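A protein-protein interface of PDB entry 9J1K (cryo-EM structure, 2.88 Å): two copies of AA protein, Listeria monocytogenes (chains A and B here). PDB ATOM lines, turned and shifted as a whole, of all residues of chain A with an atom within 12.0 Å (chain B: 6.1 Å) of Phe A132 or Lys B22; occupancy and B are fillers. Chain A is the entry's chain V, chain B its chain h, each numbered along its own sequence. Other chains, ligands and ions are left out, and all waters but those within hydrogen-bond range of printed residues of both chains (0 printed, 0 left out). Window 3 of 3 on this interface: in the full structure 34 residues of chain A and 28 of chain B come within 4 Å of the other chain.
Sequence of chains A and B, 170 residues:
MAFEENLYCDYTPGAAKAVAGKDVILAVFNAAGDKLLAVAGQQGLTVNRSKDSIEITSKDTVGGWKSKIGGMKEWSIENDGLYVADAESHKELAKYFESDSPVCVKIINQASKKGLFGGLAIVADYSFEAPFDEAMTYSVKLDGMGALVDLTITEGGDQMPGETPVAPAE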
ATOM      1  N   LEU A  82     -23.602  -9.616 -31.842  1.00  0.00           N
ATOM      2  CA  LEU A  82     -24.332  -9.083 -30.701  1.00  0.00           C
ATOM      3  C   LEU A  82     -23.946  -9.829 -29.430  1.00  0.00           C
ATOM      4  O   LEU A  82     -23.806 -11.055 -29.431  1.00  0.00           O
ATOM      5  CB  LEU A  82     -25.838  -9.192 -30.933  1.00  0.00           C
ATOM      6  CG  LEU A  82     -26.459  -8.158 -31.874  1.00  0.00           C
ATOM      7  CD1 LEU A  82     -27.963  -8.357 -31.973  1.00  0.00           C
ATOM      8  CD2 LEU A  82     -26.131  -6.746 -31.417  1.00  0.00           C
ATOM      9  N   TYR A  83     -23.784  -9.084 -28.341  1.00  0.00           N
ATOM     10  CA  TYR A  83     -23.331  -9.637 -27.072  1.00  0.00           C
ATOM     11  C   TYR A  83     -24.478  -9.667 -26.074  1.00  0.00           C
ATOM     12  O   TYR A  83     -25.198  -8.676 -25.915  1.00  0.00           O
ATOM     13  CB  TYR A  83     -22.170  -8.821 -26.498  1.00  0.00           C
ATOM     14  CG  TYR A  83     -21.699  -9.311 -25.148  1.00  0.00           C
ATOM     15  CD1 TYR A  83     -21.261 -10.615 -24.977  1.00  0.00           C
ATOM     16  CD2 TYR A  83     -21.694  -8.470 -24.043  1.00  0.00           C
ATOM     17  CE1 TYR A  83     -20.830 -11.070 -23.745  1.00  0.00           C
ATOM     18  CE2 TYR A  83     -21.265  -8.915 -22.808  1.00  0.00           C
ATOM     19  CZ  TYR A  83     -20.834 -10.216 -22.664  1.00  0.00           C
ATOM     20  OH  TYR A  83     -20.405 -10.664 -21.437  1.00  0.00           O
ATOM     21  N   PHE A 128     -15.464  -5.672 -26.173  1.00  0.00           N
ATOM     22  CA  PHE A 128     -16.823  -5.202 -26.387  1.00  0.00           C
ATOM     23  C   PHE A 128     -16.807  -3.702 -26.644  1.00  0.00           C
ATOM     24  O   PHE A 128     -15.913  -2.987 -26.186  1.00  0.00           O
ATOM     25  CB  PHE A 128     -17.726  -5.515 -25.186  1.00  0.00           C
ATOM     26  CG  PHE A 128     -17.530  -6.893 -24.622  1.00  0.00           C
ATOM     27  CD1 PHE A 128     -18.048  -7.999 -25.269  1.00  0.00           C
ATOM     28  CD2 PHE A 128     -16.826  -7.083 -23.445  1.00  0.00           C
ATOM     29  CE1 PHE A 128     -17.870  -9.268 -24.754  1.00  0.00           C
ATOM     30  CE2 PHE A 128     -16.644  -8.348 -22.927  1.00  0.00           C
ATOM     31  CZ  PHE A 128     -17.167  -9.443 -23.582  1.00  0.00           C
ATOM     32  N   GLU A 129     -17.812  -3.234 -27.383  1.00  0.00           N
ATOM     33  CA  GLU A 129     -17.985  -1.819 -27.682  1.00  0.00           C
ATOM     34  C   GLU A 129     -19.412  -1.412 -27.347  1.00  0.00           C
ATOM     35  O   GLU A 129     -20.351  -2.183 -27.566  1.00  0.00           O
ATOM     36  CB  GLU A 129     -17.685  -1.516 -29.155  1.00  0.00           C
ATOM     37  CG  GLU A 129     -16.312  -1.974 -29.617  1.00  0.00           C
ATOM     38  CD  GLU A 129     -16.383  -3.117 -30.611  1.00  0.00           C
ATOM     39  OE1 GLU A 129     -17.338  -3.148 -31.415  1.00  0.00           O
ATOM     40  OE2 GLU A 129     -15.484  -3.982 -30.587  1.00  0.00           O
ATOM     41  N   ALA A 130     -19.574  -0.193 -26.832  1.00  0.00           N
ATOM     42  CA  ALA A 130     -20.864   0.295 -26.342  1.00  0.00           C
ATOM     43  C   ALA A 130     -21.191   1.648 -26.958  1.00  0.00           C
ATOM     44  O   ALA A 130     -21.090   2.688 -26.292  1.00  0.00           O
ATOM     45  CB  ALA A 130     -20.867   0.389 -24.816  1.00  0.00           C
ATOM     46  N   PRO A 131     -21.586   1.678 -28.229  1.00  0.00           N
ATOM     47  CA  PRO A 131     -22.098   2.925 -28.802  1.00  0.00           C
ATOM     48  C   PRO A 131     -23.488   3.233 -28.273  1.00  0.00           C
ATOM     49  O   PRO A 131     -24.272   2.335 -27.956  1.00  0.00           O
ATOM     50  CB  PRO A 131     -22.125   2.640 -30.307  1.00  0.00           C
ATOM     51  CG  PRO A 131     -22.293   1.164 -30.397  1.00  0.00           C
ATOM     52  CD  PRO A 131     -21.577   0.578 -29.210  1.00  0.00           C
ATOM     53  N   PHE A 132     -23.796   4.524 -28.184  1.00  0.00           N
ATOM     54  CA  PHE A 132     -25.105   4.965 -27.722  1.00  0.00           C
ATOM     55  C   PHE A 132     -26.109   5.122 -28.854  1.00  0.00           C
ATOM     56  O   PHE A 132     -27.201   5.650 -28.625  1.00  0.00           O
ATOM     57  CB  PHE A 132     -24.989   6.285 -26.955  1.00  0.00           C
ATOM     58  CG  PHE A 132     -24.869   6.115 -25.467  1.00  0.00           C
ATOM     59  CD1 PHE A 132     -24.187   5.036 -24.930  1.00  0.00           C
ATOM     60  CD2 PHE A 132     -25.445   7.034 -24.605  1.00  0.00           C
ATOM     61  CE1 PHE A 132     -24.076   4.881 -23.561  1.00  0.00           C
ATOM     62  CE2 PHE A 132     -25.340   6.882 -23.235  1.00  0.00           C
ATOM     63  CZ  PHE A 132     -24.654   5.804 -22.713  1.00  0.00           C
ATOM     64  N   ASP A 133     -25.758   4.709 -30.070  1.00  0.00           N
ATOM     65  CA  ASP A 133     -26.692   4.684 -31.187  1.00  0.00           C
ATOM     66  C   ASP A 133     -26.926   3.273 -31.707  1.00  0.00           C
ATOM     67  O   ASP A 133     -27.633   3.097 -32.705  1.00  0.00           O
ATOM     68  CB  ASP A 133     -26.193   5.588 -32.317  1.00  0.00           C
ATOM     69  CG  ASP A 133     -24.962   5.036 -33.004  1.00  0.00           C
ATOM     70  OD1 ASP A 133     -24.114   4.431 -32.314  1.00  0.00           O
ATOM     71  OD2 ASP A 133     -24.841   5.207 -34.235  1.00  0.00           O
ATOM     72  N   GLU A 134     -26.351   2.265 -31.056  1.00  0.00           N
ATOM     73  CA  GLU A 134     -26.499   0.877 -31.467  1.00  0.00           C
ATOM     74  C   GLU A 134     -26.576   0.016 -30.210  1.00  0.00           C
ATOM     75  O   GLU A 134     -26.752   0.520 -29.097  1.00  0.00           O
ATOM     76  CB  GLU A 134     -25.351   0.461 -32.396  1.00  0.00           C
ATOM     77  CG  GLU A 134     -25.656   0.652 -33.870  1.00  0.00           C
ATOM     78  CD  GLU A 134     -24.418   0.967 -34.682  1.00  0.00           C
ATOM     79  OE1 GLU A 134     -23.301   0.834 -34.140  1.00  0.00           O
ATOM     80  OE2 GLU A 134     -24.561   1.348 -35.863  1.00  0.00           O
ATOM     81  N   ALA A 135     -26.442  -1.293 -30.389  1.00  0.00           N
ATOM     82  CA  ALA A 135     -26.580  -2.251 -29.303  1.00  0.00           C
ATOM     83  C   ALA A 135     -25.219  -2.781 -28.862  1.00  0.00           C
ATOM     84  O   ALA A 135     -24.176  -2.467 -29.442  1.00  0.00           O
ATOM     85  CB  ALA A 135     -27.492  -3.408 -29.724  1.00  0.00           C
ATOM     86  N   MET A 136     -25.247  -3.592 -27.806  1.00  0.00           N
ATOM     87  CA  MET A 136     -24.035  -4.218 -27.294  1.00  0.00           C
ATOM     88  C   MET A 136     -23.424  -5.134 -28.345  1.00  0.00           C
ATOM     89  O   MET A 136     -24.127  -5.921 -28.985  1.00  0.00           O
ATOM     90  CB  MET A 136     -24.354  -5.012 -26.025  1.00  0.00           C
ATOM     91  CG  MET A 136     -23.169  -5.587 -25.223  1.00  0.00           C
ATOM     92  SD  MET A 136     -21.622  -4.705 -24.846  1.00  0.00           S
ATOM     93  CE  MET A 136     -22.022  -2.968 -25.003  1.00  0.00           C
ATOM     94  N   THR A 137     -22.109  -5.034 -28.521  1.00  0.00           N
ATOM     95  CA  THR A 137     -21.393  -5.836 -29.500  1.00  0.00           C
ATOM     96  C   THR A 137     -20.184  -6.490 -28.849  1.00  0.00           C
ATOM     97  O   THR A 137     -19.564  -5.930 -27.943  1.00  0.00           O
ATOM     98  CB  THR A 137     -20.938  -4.995 -30.703  1.00  0.00           C
ATOM     99  OG1 THR A 137     -20.188  -3.864 -30.243  1.00  0.00           O
ATOM    100  CG2 THR A 137     -22.138  -4.515 -31.504  1.00  0.00           C
ATOM    101  N   ALA B  20     -29.068  -2.967 -25.342  1.00  0.00           N
ATOM    102  CA  ALA B  20     -28.893  -1.638 -25.908  1.00  0.00           C
ATOM    103  C   ALA B  20     -27.622  -0.996 -25.371  1.00  0.00           C
ATOM    104  O   ALA B  20     -27.276  -1.150 -24.196  1.00  0.00           O
ATOM    105  CB  ALA B  20     -30.103  -0.760 -25.593  1.00  0.00           C
ATOM    106  N   GLY B  21     -26.923  -0.269 -26.242  1.00  0.00           N
ATOM    107  CA  GLY B  21     -25.706   0.408 -25.835  1.00  0.00           C
ATOM    108  C   GLY B  21     -25.920   1.568 -24.889  1.00  0.00           C
ATOM    109  O   GLY B  21     -24.961   1.997 -24.239  1.00  0.00           O
ATOM    110  N   LYS B  22     -27.150   2.080 -24.796  1.00  0.00           N
ATOM    111  CA  LYS B  22     -27.428   3.187 -23.887  1.00  0.00           C
ATOM    112  C   LYS B  22     -27.195   2.781 -22.440  1.00  0.00           C
ATOM    113  O   LYS B  22     -26.728   3.585 -21.626  1.00  0.00           O
ATOM    114  CB  LYS B  22     -28.869   3.667 -24.063  1.00  0.00           C
ATOM    115  CG  LYS B  22     -29.511   3.296 -25.389  1.00  0.00           C
ATOM    116  CD  LYS B  22     -28.957   4.123 -26.530  1.00  0.00           C
ATOM    117  CE  LYS B  22     -29.719   3.850 -27.813  1.00  0.00           C
ATOM    118  NZ  LYS B  22     -29.699   5.024 -28.726  1.00  0.00           N
ATOM    119  N   ASP B  23     -27.515   1.535 -22.103  1.00  0.00           N
ATOM    120  CA  ASP B  23     -27.586   1.090 -20.721  1.00  0.00           C
ATOM    121  C   ASP B  23     -26.254   0.611 -20.158  1.00  0.00           C
ATOM    122  O   ASP B  23     -26.198   0.255 -18.978  1.00  0.00           O
ATOM    123  CB  ASP B  23     -28.633  -0.017 -20.589  1.00  0.00           C
ATOM    124  CG  ASP B  23     -29.990   0.402 -21.114  1.00  0.00           C
ATOM    125  OD1 ASP B  23     -30.549   1.385 -20.585  1.00  0.00           O
ATOM    126  OD2 ASP B  23     -30.498  -0.248 -22.050  1.00  0.00           O
ATOM    127  N   VAL B  24     -25.185   0.608 -20.947  1.00  0.00           N
ATOM    128  CA  VAL B  24     -23.869   0.203 -20.463  1.00  0.00           C
ATOM    129  C   VAL B  24     -23.117   1.446 -20.000  1.00  0.00           C
ATOM    130  O   VAL B  24     -22.718   2.282 -20.819  1.00  0.00           O
ATOM    131  CB  VAL B  24     -23.086  -0.552 -21.547  1.00  0.00           C
ATOM    132  CG1 VAL B  24     -21.979  -1.384 -20.918  1.00  0.00           C
ATOM    133  CG2 VAL B  24     -24.030  -1.438 -22.356  1.00  0.00           C
ATOM    134  N   ILE B  25     -22.906   1.559 -18.688  1.00  0.00           N
ATOM    135  CA  ILE B  25     -22.365   2.764 -18.066  1.00  0.00           C
ATOM    136  C   ILE B  25     -21.004   2.449 -17.460  1.00  0.00           C
ATOM    137  O   ILE B  25     -20.827   1.414 -16.804  1.00  0.00           O
ATOM    138  CB  ILE B  25     -23.302   3.354 -16.985  1.00  0.00           C
ATOM    139  CG1 ILE B  25     -24.525   4.087 -17.575  1.00  0.00           C
ATOM    140  CG2 ILE B  25     -22.537   4.312 -16.080  1.00  0.00           C
ATOM    141  CD1 ILE B  25     -25.336   3.360 -18.602  1.00  0.00           C
ATOM    142  N   GLN B  42     -21.316  10.418 -21.098  1.00  0.00           N
ATOM    143  CA  GLN B  42     -20.810   9.135 -21.573  1.00  0.00           C
ATOM    144  C   GLN B  42     -21.467   8.796 -22.905  1.00  0.00           C
ATOM    145  O   GLN B  42     -22.580   8.262 -22.941  1.00  0.00           O
ATOM    146  CB  GLN B  42     -21.078   8.054 -20.532  1.00  0.00           C
ATOM    147  CG  GLN B  42     -20.146   6.863 -20.620  1.00  0.00           C
ATOM    148  CD  GLN B  42     -20.447   5.814 -19.570  1.00  0.00           C
ATOM    149  OE1 GLN B  42     -20.458   4.618 -19.857  1.00  0.00           O
ATOM    150  NE2 GLN B  42     -20.700   6.258 -18.345  1.00  0.00           N
ATOM    151  N   GLN B  43     -20.778   9.101 -24.003  1.00  0.00           N
ATOM    152  CA  GLN B  43     -21.332   8.930 -25.341  1.00  0.00           C
ATOM    153  C   GLN B  43     -20.969   7.561 -25.902  1.00  0.00           C
ATOM    154  O   GLN B  43     -21.850   6.753 -26.211  1.00  0.00           O
ATOM    155  CB  GLN B  43     -20.821  10.049 -26.254  1.00  0.00           C
ATOM    156  CG  GLN B  43     -21.488  10.202 -27.618  1.00  0.00           C
ATOM    157  CD  GLN B  43     -22.905   9.674 -27.668  1.00  0.00           C
ATOM    158  OE1 GLN B  43     -23.130   8.496 -27.927  1.00  0.00           O
ATOM    159  NE2 GLN B  43     -23.872  10.548 -27.413  1.00  0.00           N
ATOM    160  N   GLY B  44     -19.670   7.285 -26.023  1.00  0.00           N
ATOM    161  CA  GLY B  44     -19.214   6.007 -26.517  1.00  0.00           C
ATOM    162  C   GLY B  44     -18.156   5.377 -25.628  1.00  0.00           C
ATOM    163  O   GLY B  44     -17.411   6.065 -24.928  1.00  0.00           O
ATOM    164  N   GLN B 110     -27.593  -0.378 -16.295  1.00  0.00           N
ATOM    165  CA  GLN B 110     -28.689   0.091 -15.448  1.00  0.00           C
ATOM    166  C   GLN B 110     -29.955  -0.724 -15.672  1.00  0.00           C
ATOM    167  O   GLN B 110     -30.663  -1.039 -14.709  1.00  0.00           O
ATOM    168  CB  GLN B 110     -29.022   1.569 -15.681  1.00  0.00           C
ATOM    169  CG  GLN B 110     -29.247   2.006 -17.127  1.00  0.00           C
ATOM    170  CD  GLN B 110     -28.558   3.309 -17.485  1.00  0.00           C
ATOM    171  OE1 GLN B 110     -28.268   4.136 -16.613  1.00  0.00           O
ATOM    172  NE2 GLN B 110     -28.375   3.538 -18.780  1.00  0.00           N
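O of Ala A130 touches CA of Gly B44, 3.8 Å away.
Gly B21 touches Pro A131 (CA to O, 3.2 Å).
Gly B21 touches Phe A132 (O to CE1, 3.1 Å).
Gln B42 touches Phe A132.
CB of Phe A132 touches OE1 of Gln B43, 3.0 Å away.
NZ of Lys B22 touches CA of Asp A133, 3.9 Å away.
N of Gly B21 touches CA of Ala A135 (3.7 Å).
Met A136 touches Val B24.
No residue of chain A comes within 4 Å of Ala B20.
Of chain A, only Pro A131, Phe A132, Glu A134 and Ala A135 come within 4 Å of Gly B21.
No residue of chain A comes within 4 Å of Asp B23.
Of chain A, only Phe A132 (3.1 Å) comes within 4 Å of Gln B42.
Gln B43 touches one residue of chain A.
Of chain A, only Ala A130 (3.8 Å) comes within 4 Å of Gly B44.
Printed residues of chain B within 4 Å of Met A136: Val B24 (3.7 Å).
Of the printed residues of chain B, Asp A133 touches Lys B22 (3.9 Å).
Of the printed residues of chain B, Pro A131 touches Gly B21.
Glu A129 touches none of the printed residues of chain B.
No position is printed for both chains.
Printed residues of chain B that touch a printed residue of chain A: Gly B21, Lys B22, Val B24, Gln B42, Gln B43 and Gly B44.
Printed residues of chain A that touch a printed residue of chain B: Ala A130, Pro A131, Phe A132, Asp A133, Glu A134, Ala A135 and Met A136.
Hydrophobic or aromatic side chains of chain A within 4 Å of the printed part of chain B: Phe A132 and Met A136.
O of Phe A132 lies within hydrogen-bond range of NZ of Lys B22 (2.6 Å).
The backbone carbonyl oxygen (O) of Glu A134 lies within hydrogen-bond range of the backbone NH (N) of Gly B21, 3.0 Å away.
O of Met A136 lies within hydrogen-bond range of N of Tyr A83, 3.2 Å away.
The backbone carbonyl oxygen (O) of Lys B22 is in hydrogen-bond range of the side-chain amide nitrogen (NE2) of Gln B110, at 3.3 Å.
The backbone carbonyl oxygen (O) of Val B24 lies close to the side-chain amide oxygen (OE1) of Gln B42 (3.4 Å).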
